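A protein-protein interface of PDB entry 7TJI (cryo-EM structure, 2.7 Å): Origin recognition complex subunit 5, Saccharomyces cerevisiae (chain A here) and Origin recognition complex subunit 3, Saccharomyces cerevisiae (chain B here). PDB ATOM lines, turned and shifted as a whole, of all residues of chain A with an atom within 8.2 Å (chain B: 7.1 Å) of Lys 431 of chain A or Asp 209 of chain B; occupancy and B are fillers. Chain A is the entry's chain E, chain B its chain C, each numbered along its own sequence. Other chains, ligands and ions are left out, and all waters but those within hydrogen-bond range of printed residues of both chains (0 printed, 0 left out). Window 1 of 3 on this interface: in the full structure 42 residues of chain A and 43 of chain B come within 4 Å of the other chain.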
ATOM      1  N   LEU A 332     -15.078 -18.296 -17.001  1.00  0.00           N
ATOM      2  CA  LEU A 332     -14.590 -19.515 -16.355  1.00  0.00           C
ATOM      3  C   LEU A 332     -15.641 -20.124 -15.433  1.00  0.00           C
ATOM      4  O   LEU A 332     -15.796 -21.353 -15.387  1.00  0.00           O
ATOM      5  CB  LEU A 332     -13.309 -19.221 -15.578  1.00  0.00           C
ATOM      6  CG  LEU A 332     -12.012 -19.731 -16.207  1.00  0.00           C
ATOM      7  CD1 LEU A 332     -10.821 -19.487 -15.298  1.00  0.00           C
ATOM      8  CD2 LEU A 332     -12.121 -21.202 -16.560  1.00  0.00           C
ATOM      9  N   LEU A 424     -12.515 -15.422 -24.233  1.00  0.00           N
ATOM     10  CA  LEU A 424     -12.653 -16.870 -24.361  1.00  0.00           C
ATOM     11  C   LEU A 424     -11.473 -17.480 -25.116  1.00  0.00           C
ATOM     12  O   LEU A 424     -10.974 -18.555 -24.745  1.00  0.00           O
ATOM     13  CB  LEU A 424     -13.975 -17.188 -25.054  1.00  0.00           C
ATOM     14  CG  LEU A 424     -14.505 -18.617 -25.169  1.00  0.00           C
ATOM     15  CD1 LEU A 424     -14.295 -19.423 -23.900  1.00  0.00           C
ATOM     16  CD2 LEU A 424     -15.972 -18.555 -25.529  1.00  0.00           C
ATOM     17  N   SER A 425     -11.007 -16.795 -26.168  1.00  0.00           N
ATOM     18  CA  SER A 425      -9.817 -17.228 -26.894  1.00  0.00           C
ATOM     19  C   SER A 425      -8.580 -17.193 -26.004  1.00  0.00           C
ATOM     20  O   SER A 425      -7.723 -18.085 -26.081  1.00  0.00           O
ATOM     21  CB  SER A 425      -9.619 -16.345 -28.125  1.00  0.00           C
ATOM     22  OG  SER A 425      -8.990 -17.050 -29.178  1.00  0.00           O
ATOM     23  N   GLU A 426      -8.473 -16.166 -25.155  1.00  0.00           N
ATOM     24  CA  GLU A 426      -7.366 -16.098 -24.208  1.00  0.00           C
ATOM     25  C   GLU A 426      -7.434 -17.226 -23.188  1.00  0.00           C
ATOM     26  O   GLU A 426      -6.403 -17.810 -22.839  1.00  0.00           O
ATOM     27  CB  GLU A 426      -7.354 -14.740 -23.507  1.00  0.00           C
ATOM     28  CG  GLU A 426      -6.058 -14.432 -22.776  1.00  0.00           C
ATOM     29  CD  GLU A 426      -4.819 -14.663 -23.621  1.00  0.00           C
ATOM     30  OE1 GLU A 426      -4.769 -14.170 -24.770  1.00  0.00           O
ATOM     31  OE2 GLU A 426      -3.889 -15.341 -23.136  1.00  0.00           O
ATOM     32  N   LEU A 427      -8.644 -17.554 -22.716  1.00  0.00           N
ATOM     33  CA  LEU A 427      -8.830 -18.668 -21.789  1.00  0.00           C
ATOM     34  C   LEU A 427      -8.409 -19.989 -22.417  1.00  0.00           C
ATOM     35  O   LEU A 427      -7.844 -20.853 -21.738  1.00  0.00           O
ATOM     36  CB  LEU A 427     -10.290 -18.743 -21.335  1.00  0.00           C
ATOM     37  CG  LEU A 427     -10.760 -17.751 -20.270  1.00  0.00           C
ATOM     38  CD1 LEU A 427     -12.252 -17.871 -20.046  1.00  0.00           C
ATOM     39  CD2 LEU A 427     -10.011 -17.969 -18.972  1.00  0.00           C
ATOM     40  N   HIS A 428      -8.672 -20.161 -23.716  1.00  0.00           N
ATOM     41  CA  HIS A 428      -8.123 -21.321 -24.411  1.00  0.00           C
ATOM     42  C   HIS A 428      -6.602 -21.249 -24.528  1.00  0.00           C
ATOM     43  O   HIS A 428      -5.935 -22.289 -24.494  1.00  0.00           O
ATOM     44  CB  HIS A 428      -8.751 -21.474 -25.792  1.00  0.00           C
ATOM     45  CG  HIS A 428      -8.343 -22.730 -26.497  1.00  0.00           C
ATOM     46  ND1 HIS A 428      -7.237 -22.800 -27.315  1.00  0.00           N
ATOM     47  CD2 HIS A 428      -8.877 -23.973 -26.483  1.00  0.00           C
ATOM     48  CE1 HIS A 428      -7.117 -24.027 -27.787  1.00  0.00           C
ATOM     49  NE2 HIS A 428      -8.100 -24.759 -27.297  1.00  0.00           N
ATOM     50  N   THR A 429      -6.039 -20.045 -24.668  1.00  0.00           N
ATOM     51  CA  THR A 429      -4.584 -19.912 -24.715  1.00  0.00           C
ATOM     52  C   THR A 429      -3.948 -20.226 -23.359  1.00  0.00           C
ATOM     53  O   THR A 429      -2.935 -20.933 -23.294  1.00  0.00           O
ATOM     54  CB  THR A 429      -4.207 -18.508 -25.207  1.00  0.00           C
ATOM     55  OG1 THR A 429      -4.529 -18.390 -26.597  1.00  0.00           O
ATOM     56  CG2 THR A 429      -2.718 -18.215 -25.022  1.00  0.00           C
ATOM     57  N   LEU A 430      -4.557 -19.770 -22.259  1.00  0.00           N
ATOM     58  CA  LEU A 430      -4.012 -20.033 -20.926  1.00  0.00           C
ATOM     59  C   LEU A 430      -4.248 -21.458 -20.428  1.00  0.00           C
ATOM     60  O   LEU A 430      -3.924 -21.735 -19.268  1.00  0.00           O
ATOM     61  CB  LEU A 430      -4.588 -19.072 -19.878  1.00  0.00           C
ATOM     62  CG  LEU A 430      -4.558 -17.544 -19.971  1.00  0.00           C
ATOM     63  CD1 LEU A 430      -5.945 -16.962 -19.773  1.00  0.00           C
ATOM     64  CD2 LEU A 430      -3.597 -16.968 -18.961  1.00  0.00           C
ATOM     65  N   LYS A 431      -4.846 -22.334 -21.246  1.00  0.00           N
ATOM     66  CA  LYS A 431      -5.170 -23.732 -20.938  1.00  0.00           C
ATOM     67  C   LYS A 431      -6.144 -23.878 -19.772  1.00  0.00           C
ATOM     68  O   LYS A 431      -6.256 -24.960 -19.188  1.00  0.00           O
ATOM     69  CB  LYS A 431      -3.909 -24.575 -20.683  1.00  0.00           C
ATOM     70  CG  LYS A 431      -3.590 -25.563 -21.777  1.00  0.00           C
ATOM     71  CD  LYS A 431      -2.783 -24.915 -22.878  1.00  0.00           C
ATOM     72  CE  LYS A 431      -2.256 -25.947 -23.858  1.00  0.00           C
ATOM     73  NZ  LYS A 431      -1.803 -25.316 -25.129  1.00  0.00           N
ATOM     74  N   LEU A 432      -6.865 -22.811 -19.420  1.00  0.00           N
ATOM     75  CA  LEU A 432      -7.935 -22.905 -18.439  1.00  0.00           C
ATOM     76  C   LEU A 432      -9.224 -23.426 -19.057  1.00  0.00           C
ATOM     77  O   LEU A 432     -10.136 -23.816 -18.324  1.00  0.00           O
ATOM     78  CB  LEU A 432      -8.169 -21.542 -17.788  1.00  0.00           C
ATOM     79  CG  LEU A 432      -6.916 -20.844 -17.253  1.00  0.00           C
ATOM     80  CD1 LEU A 432      -7.259 -19.502 -16.631  1.00  0.00           C
ATOM     81  CD2 LEU A 432      -6.182 -21.722 -16.250  1.00  0.00           C
ATOM     82  N   ILE A 433      -9.309 -23.433 -20.385  1.00  0.00           N
ATOM     83  CA  ILE A 433     -10.370 -24.083 -21.146  1.00  0.00           C
ATOM     84  C   ILE A 433      -9.696 -25.004 -22.150  1.00  0.00           C
ATOM     85  O   ILE A 433      -8.701 -24.625 -22.776  1.00  0.00           O
ATOM     86  CB  ILE A 433     -11.278 -23.059 -21.868  1.00  0.00           C
ATOM     87  CG1 ILE A 433     -11.886 -22.075 -20.879  1.00  0.00           C
ATOM     88  CG2 ILE A 433     -12.400 -23.739 -22.623  1.00  0.00           C
ATOM     89  CD1 ILE A 433     -12.820 -22.714 -19.930  1.00  0.00           C
ATOM     90  N   ALA A 434     -10.221 -26.216 -22.299  1.00  0.00           N
ATOM     91  CA  ALA A 434      -9.685 -27.171 -23.250  1.00  0.00           C
ATOM     92  C   ALA A 434     -10.760 -27.607 -24.235  1.00  0.00           C
ATOM     93  O   ALA A 434     -11.962 -27.446 -24.000  1.00  0.00           O
ATOM     94  CB  ALA A 434      -9.099 -28.397 -22.539  1.00  0.00           C
ATOM     95  N   THR A 435     -10.302 -28.141 -25.357  1.00  0.00           N
ATOM     96  CA  THR A 435     -11.131 -28.799 -26.353  1.00  0.00           C
ATOM     97  C   THR A 435     -10.804 -30.281 -26.386  1.00  0.00           C
ATOM     98  O   THR A 435      -9.898 -30.761 -25.705  1.00  0.00           O
ATOM     99  CB  THR A 435     -10.921 -28.209 -27.749  1.00  0.00           C
ATOM    100  OG1 THR A 435      -9.523 -28.005 -27.981  1.00  0.00           O
ATOM    101  CG2 THR A 435     -11.662 -26.926 -27.909  1.00  0.00           C
ATOM    102  N   ASN A 438      -6.467 -30.888 -29.708  1.00  0.00           N
ATOM    103  CA  ASN A 438      -5.373 -30.129 -29.127  1.00  0.00           C
ATOM    104  C   ASN A 438      -4.403 -29.570 -30.156  1.00  0.00           C
ATOM    105  O   ASN A 438      -3.828 -28.506 -29.922  1.00  0.00           O
ATOM    106  CB  ASN A 438      -4.605 -30.998 -28.122  1.00  0.00           C
ATOM    107  CG  ASN A 438      -5.524 -31.903 -27.318  1.00  0.00           C
ATOM    108  OD1 ASN A 438      -5.902 -32.985 -27.770  1.00  0.00           O
ATOM    109  ND2 ASN A 438      -5.894 -31.459 -26.124  1.00  0.00           N
ATOM    110  N   TYR A 443     -11.327 -23.434 -34.292  1.00  0.00           N
ATOM    111  CA  TYR A 443     -12.278 -22.933 -33.309  1.00  0.00           C
ATOM    112  C   TYR A 443     -13.693 -22.836 -33.853  1.00  0.00           C
ATOM    113  O   TYR A 443     -14.647 -22.839 -33.070  1.00  0.00           O
ATOM    114  CB  TYR A 443     -11.835 -21.554 -32.826  1.00  0.00           C
ATOM    115  CG  TYR A 443     -10.558 -21.567 -32.031  1.00  0.00           C
ATOM    116  CD1 TYR A 443     -10.473 -22.269 -30.835  1.00  0.00           C
ATOM    117  CD2 TYR A 443      -9.430 -20.886 -32.478  1.00  0.00           C
ATOM    118  CE1 TYR A 443      -9.305 -22.287 -30.103  1.00  0.00           C
ATOM    119  CE2 TYR A 443      -8.255 -20.898 -31.750  1.00  0.00           C
ATOM    120  CZ  TYR A 443      -8.200 -21.605 -30.566  1.00  0.00           C
ATOM    121  OH  TYR A 443      -7.039 -21.623 -29.835  1.00  0.00           O
ATOM    122  N   LYS A 451     -14.574 -27.741 -22.747  1.00  0.00           N
ATOM    123  CA  LYS A 451     -14.647 -28.164 -21.359  1.00  0.00           C
ATOM    124  C   LYS A 451     -13.732 -27.273 -20.536  1.00  0.00           C
ATOM    125  O   LYS A 451     -12.793 -26.665 -21.054  1.00  0.00           O
ATOM    126  CB  LYS A 451     -14.277 -29.644 -21.187  1.00  0.00           C
ATOM    127  CG  LYS A 451     -12.822 -29.973 -21.447  1.00  0.00           C
ATOM    128  CD  LYS A 451     -12.599 -31.475 -21.529  1.00  0.00           C
ATOM    129  CE  LYS A 451     -11.223 -31.792 -22.081  1.00  0.00           C
ATOM    130  NZ  LYS A 451     -11.019 -33.248 -22.290  1.00  0.00           N
ATOM    131  N   VAL A 452     -14.036 -27.175 -19.262  1.00  0.00           N
ATOM    132  CA  VAL A 452     -13.171 -26.466 -18.330  1.00  0.00           C
ATOM    133  C   VAL A 452     -12.125 -27.451 -17.824  1.00  0.00           C
ATOM    134  O   VAL A 452     -12.388 -28.655 -17.722  1.00  0.00           O
ATOM    135  CB  VAL A 452     -13.999 -25.826 -17.188  1.00  0.00           C
ATOM    136  CG1 VAL A 452     -14.580 -26.855 -16.226  1.00  0.00           C
ATOM    137  CG2 VAL A 452     -13.194 -24.788 -16.442  1.00  0.00           C
ATOM    138  N   ASN A 453     -10.897 -26.973 -17.609  1.00  0.00           N
ATOM    139  CA  ASN A 453      -9.919 -27.729 -16.827  1.00  0.00           C
ATOM    140  C   ASN A 453      -9.309 -26.784 -15.795  1.00  0.00           C
ATOM    141  O   ASN A 453      -8.207 -26.256 -15.961  1.00  0.00           O
ATOM    142  CB  ASN A 453      -8.848 -28.410 -17.719  1.00  0.00           C
ATOM    143  CG  ASN A 453      -8.246 -27.478 -18.752  1.00  0.00           C
ATOM    144  OD1 ASN A 453      -8.893 -26.548 -19.224  1.00  0.00           O
ATOM    145  ND2 ASN A 453      -6.990 -27.726 -19.102  1.00  0.00           N
ATOM    146  N   VAL A 454     -10.040 -26.590 -14.702  1.00  0.00           N
ATOM    147  CA  VAL A 454      -9.505 -26.030 -13.466  1.00  0.00           C
ATOM    148  C   VAL A 454      -9.998 -26.950 -12.355  1.00  0.00           C
ATOM    149  O   VAL A 454     -11.021 -27.631 -12.530  1.00  0.00           O
ATOM    150  CB  VAL A 454      -9.935 -24.567 -13.234  1.00  0.00           C
ATOM    151  CG1 VAL A 454      -9.321 -23.628 -14.273  1.00  0.00           C
ATOM    152  CG2 VAL A 454     -11.446 -24.431 -13.192  1.00  0.00           C
ATOM    153  N   SER B 110       3.621 -12.603 -17.202  1.00  0.00           N
ATOM    154  CA  SER B 110       4.584 -12.393 -18.270  1.00  0.00           C
ATOM    155  C   SER B 110       3.986 -12.864 -19.586  1.00  0.00           C
ATOM    156  O   SER B 110       3.363 -13.928 -19.644  1.00  0.00           O
ATOM    157  CB  SER B 110       5.888 -13.137 -17.979  1.00  0.00           C
ATOM    158  OG  SER B 110       6.779 -13.052 -19.075  1.00  0.00           O
ATOM    159  N   PRO B 133       6.695 -23.747 -26.096  1.00  0.00           N
ATOM    160  CA  PRO B 133       5.972 -25.032 -26.047  1.00  0.00           C
ATOM    161  C   PRO B 133       5.980 -25.818 -27.370  1.00  0.00           C
ATOM    162  O   PRO B 133       5.909 -27.002 -27.342  1.00  0.00           O
ATOM    163  CB  PRO B 133       4.582 -24.540 -25.601  1.00  0.00           C
ATOM    164  CG  PRO B 133       4.470 -23.137 -26.093  1.00  0.00           C
ATOM    165  CD  PRO B 133       5.850 -22.578 -25.871  1.00  0.00           C
ATOM    166  N   LYS B 206       9.225 -20.037 -22.162  1.00  0.00           N
ATOM    167  CA  LYS B 206       8.146 -19.103 -22.577  1.00  0.00           C
ATOM    168  C   LYS B 206       6.818 -19.862 -22.667  1.00  0.00           C
ATOM    169  O   LYS B 206       6.834 -21.013 -23.145  1.00  0.00           O
ATOM    170  CB  LYS B 206       8.510 -18.464 -23.920  1.00  0.00           C
ATOM    171  CG  LYS B 206       9.894 -17.832 -23.974  1.00  0.00           C
ATOM    172  CD  LYS B 206      10.327 -17.464 -25.375  1.00  0.00           C
ATOM    173  CE  LYS B 206       9.344 -16.552 -26.076  1.00  0.00           C
ATOM    174  NZ  LYS B 206       9.799 -16.202 -27.442  1.00  0.00           N
ATOM    175  N   ASP B 207       5.720 -19.241 -22.226  1.00  0.00           N
ATOM    176  CA  ASP B 207       4.374 -19.872 -22.327  1.00  0.00           C
ATOM    177  C   ASP B 207       4.352 -21.198 -21.560  1.00  0.00           C
ATOM    178  O   ASP B 207       3.969 -22.220 -22.165  1.00  0.00           O
ATOM    179  CB  ASP B 207       3.964 -20.066 -23.789  1.00  0.00           C
ATOM    180  CG  ASP B 207       4.145 -18.819 -24.637  1.00  0.00           C
ATOM    181  OD1 ASP B 207       4.546 -17.781 -24.075  1.00  0.00           O
ATOM    182  OD2 ASP B 207       3.885 -18.898 -25.854  1.00  0.00           O
ATOM    183  N   VAL B 208       4.741 -21.180 -20.281  1.00  0.00           N
ATOM    184  CA  VAL B 208       4.709 -22.416 -19.443  1.00  0.00           C
ATOM    185  C   VAL B 208       3.260 -22.904 -19.346  1.00  0.00           C
ATOM    186  O   VAL B 208       3.040 -24.122 -19.492  1.00  0.00           O
ATOM    187  CB  VAL B 208       5.310 -22.158 -18.048  1.00  0.00           C
ATOM    188  CG1 VAL B 208       5.247 -23.396 -17.168  1.00  0.00           C
ATOM    189  CG2 VAL B 208       6.736 -21.634 -18.137  1.00  0.00           C
ATOM    190  N   ASP B 209       2.314 -21.992 -19.107  1.00  0.00           N
ATOM    191  CA  ASP B 209       0.909 -22.353 -19.003  1.00  0.00           C
ATOM    192  C   ASP B 209       0.425 -23.173 -20.193  1.00  0.00           C
ATOM    193  O   ASP B 209      -0.535 -23.936 -20.052  1.00  0.00           O
ATOM    194  CB  ASP B 209       0.085 -21.080 -18.851  1.00  0.00           C
ATOM    195  CG  ASP B 209       0.006 -20.620 -17.419  1.00  0.00           C
ATOM    196  OD1 ASP B 209      -0.152 -21.482 -16.527  1.00  0.00           O
ATOM    197  OD2 ASP B 209       0.110 -19.400 -17.181  1.00  0.00           O
ATOM    198  N   SER B 210       1.076 -23.046 -21.350  1.00  0.00           N
ATOM    199  CA  SER B 210       0.750 -23.835 -22.529  1.00  0.00           C
ATOM    200  C   SER B 210       1.611 -25.083 -22.683  1.00  0.00           C
ATOM    201  O   SER B 210       1.330 -25.899 -23.566  1.00  0.00           O
ATOM    202  CB  SER B 210       0.884 -22.974 -23.790  1.00  0.00           C
ATOM    203  OG  SER B 210       0.297 -23.614 -24.910  1.00  0.00           O
ATOM    204  N   ILE B 211       2.636 -25.260 -21.853  1.00  0.00           N
ATOM    205  CA  ILE B 211       3.529 -26.404 -21.997  1.00  0.00           C
ATOM    206  C   ILE B 211       2.906 -27.639 -21.350  1.00  0.00           C
ATOM    207  O   ILE B 211       2.020 -27.555 -20.494  1.00  0.00           O
ATOM    208  CB  ILE B 211       4.924 -26.092 -21.409  1.00  0.00           C
ATOM    209  CG1 ILE B 211       6.024 -26.744 -22.247  1.00  0.00           C
ATOM    210  CG2 ILE B 211       5.052 -26.535 -19.949  1.00  0.00           C
ATOM    211  CD1 ILE B 211       7.421 -26.474 -21.736  1.00  0.00           C
ATOM    212  N   ASN B 212       3.358 -28.809 -21.798  1.00  0.00           N
ATOM    213  CA  ASN B 212       3.023 -30.063 -21.135  1.00  0.00           C
ATOM    214  C   ASN B 212       3.846 -30.177 -19.859  1.00  0.00           C
ATOM    215  O   ASN B 212       5.080 -30.236 -19.914  1.00  0.00           O
ATOM    216  CB  ASN B 212       3.291 -31.246 -22.059  1.00  0.00           C
ATOM    217  CG  ASN B 212       2.489 -32.472 -21.678  1.00  0.00           C
ATOM    218  OD1 ASN B 212       2.887 -33.241 -20.807  1.00  0.00           O
ATOM    219  ND2 ASN B 212       1.348 -32.657 -22.330  1.00  0.00           N
ATOM    220  N   PHE B 213       3.168 -30.208 -18.712  1.00  0.00           N
ATOM    221  CA  PHE B 213       3.870 -30.163 -17.434  1.00  0.00           C
ATOM    222  C   PHE B 213       4.580 -31.466 -17.106  1.00  0.00           C
ATOM    223  O   PHE B 213       5.538 -31.450 -16.328  1.00  0.00           O
ATOM    224  CB  PHE B 213       2.899 -29.784 -16.318  1.00  0.00           C
ATOM    225  CG  PHE B 213       2.582 -28.324 -16.288  1.00  0.00           C
ATOM    226  CD1 PHE B 213       3.459 -27.426 -15.701  1.00  0.00           C
ATOM    227  CD2 PHE B 213       1.431 -27.841 -16.882  1.00  0.00           C
ATOM    228  CE1 PHE B 213       3.180 -26.071 -15.688  1.00  0.00           C
ATOM    229  CE2 PHE B 213       1.146 -26.486 -16.874  1.00  0.00           C
ATOM    230  CZ  PHE B 213       2.020 -25.602 -16.275  1.00  0.00           C
ATOM    231  N   ASN B 239       8.027 -17.992 -17.194  1.00  0.00           N
ATOM    232  CA  ASN B 239       7.094 -16.919 -17.527  1.00  0.00           C
ATOM    233  C   ASN B 239       5.680 -17.428 -17.282  1.00  0.00           C
ATOM    234  O   ASN B 239       5.138 -18.195 -18.080  1.00  0.00           O
ATOM    235  CB  ASN B 239       7.285 -16.469 -18.969  1.00  0.00           C
ATOM    236  CG  ASN B 239       8.665 -15.907 -19.228  1.00  0.00           C
ATOM    237  OD1 ASN B 239       8.952 -14.766 -18.884  1.00  0.00           O
ATOM    238  ND2 ASN B 239       9.523 -16.706 -19.846  1.00  0.00           N
ATOM    239  N   ILE B 240       5.057 -16.963 -16.258  1.00  0.00           N
ATOM    240  CA  ILE B 240       3.769 -17.490 -15.782  1.00  0.00           C
ATOM    241  C   ILE B 240       2.655 -16.490 -16.051  1.00  0.00           C
ATOM    242  O   ILE B 240       2.824 -15.385 -15.778  1.00  0.00           O
ATOM    243  CB  ILE B 240       3.912 -17.904 -14.311  1.00  0.00           C
ATOM    244  CG1 ILE B 240       4.374 -19.355 -14.122  1.00  0.00           C
ATOM    245  CG2 ILE B 240       2.600 -17.714 -13.588  1.00  0.00           C
ATOM    246  CD1 ILE B 240       5.567 -19.789 -14.905  1.00  0.00           C
ATOM    247  N   ASN B 241       1.531 -16.934 -16.622  1.00  0.00           N
ATOM    248  CA  ASN B 241       0.486 -15.954 -17.034  1.00  0.00           C
ATOM    249  C   ASN B 241      -0.679 -15.907 -16.036  1.00  0.00           C
ATOM    250  O   ASN B 241      -1.374 -14.874 -16.010  1.00  0.00           O
ATOM    251  CB  ASN B 241      -0.021 -16.240 -18.451  1.00  0.00           C
ATOM    252  CG  ASN B 241      -0.692 -15.043 -19.091  1.00  0.00           C
ATOM    253  OD1 ASN B 241      -0.672 -13.944 -18.540  1.00  0.00           O
ATOM    254  ND2 ASN B 241      -1.294 -15.245 -20.252  1.00  0.00           N
ATOM    255  N   THR B 242      -0.894 -16.967 -15.254  1.00  0.00           N
ATOM    256  CA  THR B 242      -2.083 -16.996 -14.358  1.00  0.00           C
ATOM    257  C   THR B 242      -1.670 -16.785 -12.900  1.00  0.00           C
ATOM    258  O   THR B 242      -2.079 -15.758 -12.323  1.00  0.00           O
ATOM    259  CB  THR B 242      -2.847 -18.318 -14.505  1.00  0.00           C
ATOM    260  OG1 THR B 242      -2.012 -19.373 -14.025  1.00  0.00           O
ATOM    261  CG2 THR B 242      -3.260 -18.606 -15.931  1.00  0.00           C
ATOM    262  N   ASN B 243      -0.891 -17.710 -12.337  1.00  0.00           N
ATOM    263  CA  ASN B 243      -0.507 -17.651 -10.924  1.00  0.00           C
ATOM    264  C   ASN B 243       0.386 -18.851 -10.615  1.00  0.00           C
ATOM    265  O   ASN B 243       0.506 -19.784 -11.413  1.00  0.00           O
ATOM    266  CB  ASN B 243      -1.717 -17.614  -9.976  1.00  0.00           C
ATOM    267  CG  ASN B 243      -2.522 -18.891  -9.997  1.00  0.00           C
ATOM    268  OD1 ASN B 243      -2.396 -19.732  -9.108  1.00  0.00           O
ATOM    269  ND2 ASN B 243      -3.322 -19.068 -11.035  1.00  0.00           N
ATOM    270  N   ASN B 246      -1.438 -22.608  -9.639  1.00  0.00           N
ATOM    271  CA  ASN B 246      -1.891 -23.382 -10.790  1.00  0.00           C
ATOM    272  C   ASN B 246      -0.764 -24.197 -11.414  1.00  0.00           C
ATOM    273  O   ASN B 246      -1.026 -25.219 -12.057  1.00  0.00           O
ATOM    274  CB  ASN B 246      -2.502 -22.451 -11.834  1.00  0.00           C
ATOM    275  CG  ASN B 246      -3.443 -23.169 -12.774  1.00  0.00           C
ATOM    276  OD1 ASN B 246      -3.799 -24.326 -12.552  1.00  0.00           O
ATOM    277  ND2 ASN B 246      -3.852 -22.484 -13.834  1.00  0.00           N
ATOM    278  N   ILE B 247       0.485 -23.767 -11.242  1.00  0.00           N
ATOM    279  CA  ILE B 247       1.611 -24.547 -11.739  1.00  0.00           C
ATOM    280  C   ILE B 247       2.234 -25.417 -10.652  1.00  0.00           C
ATOM    281  O   ILE B 247       2.888 -26.420 -10.977  1.00  0.00           O
ATOM    282  CB  ILE B 247       2.660 -23.628 -12.404  1.00  0.00           C
ATOM    283  CG1 ILE B 247       3.783 -23.226 -11.442  1.00  0.00           C
ATOM    284  CG2 ILE B 247       1.993 -22.385 -12.976  1.00  0.00           C
ATOM    285  CD1 ILE B 247       5.141 -23.776 -11.816  1.00  0.00           C
ATOM    286  N   ASN B 250       0.558 -28.725 -10.728  1.00  0.00           N
ATOM    287  CA  ASN B 250       0.821 -29.488 -11.939  1.00  0.00           C
ATOM    288  C   ASN B 250       2.179 -30.173 -11.940  1.00  0.00           C
ATOM    289  O   ASN B 250       2.405 -31.057 -12.770  1.00  0.00           O
ATOM    290  CB  ASN B 250       0.716 -28.575 -13.164  1.00  0.00           C
ATOM    291  CG  ASN B 250      -0.695 -28.472 -13.686  1.00  0.00           C
ATOM    292  OD1 ASN B 250      -1.560 -29.269 -13.329  1.00  0.00           O
ATOM    293  ND2 ASN B 250      -0.941 -27.481 -14.529  1.00  0.00           N
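Lys 431 of chain A touches just these residues of chain B: Asp 209 and Ser 210.
Printed residues of chain A within 4 Å of Asp 209 of chain B: Lys 431.
Printed residues of chain B within 4 Å of Leu 430 of chain A: Asn 241 (3.2 Å) and Thr 242 (3.5 Å).
Of the printed residues of chain B, Glu 426 of chain A touches Asn 241 (3.9 Å).
Asn 438 of chain A touches none of the printed residues of chain B.
The nearest residue of chain A that does not touch Asp 209 of chain B is Leu 430 of chain A (4.1 Å).
N of Asn 241 of chain B sits at hydrogen-bond distance from OD2 of Asp 209 of chain B.
The side-chain carboxylate of Asp 209 of chain B lies within hydrogen-bond range of the backbone NH of Thr 242 of chain B, at 3.3 Å.
The side-chain amide nitrogen of Asn 250 of chain B lies within hydrogen-bond range of the backbone carbonyl oxygen of Asn 246 of chain B (3.4 Å).
O of Leu 427 of chain A is in hydrogen-bond range of N of Leu 432 of chain A (3.2 Å).
The backbone carbonyl oxygen of Lys 431 of chain A lies within hydrogen-bond range of the side-chain amide nitrogen of Asn 453 of chain A (2.9 Å).
OD1 of Asn 453 of chain A sits close to O of Leu 432 of chain A.
Printed residues of chain A that touch a printed residue of chain B: Glu 426, Leu 430, Lys 431 and Leu 432.
Printed residues of chain B that touch a printed residue of chain A: Asp 209, Ser 210, Asn 241, Thr 242 and Asn 246.
The side-chain hydroxyl (OG) of Ser 210 of chain B lies within hydrogen-bond range of the side-chain amino group (NZ) of Lys 431 of chain A.
Glu 426 of chain A touches Asn 241 of chain B.
Asn 241 of chain B touches Leu 430 of chain A (ND2 to CD2, 3.2 Å).
Thr 242 of chain B touches Leu 430 of chain A.
Asp 209 of chain B touches Lys 431 of chain A.
Leu 432 of chain A touches Asn 246 of chain B (CD2 to ND2, 3.4 Å).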
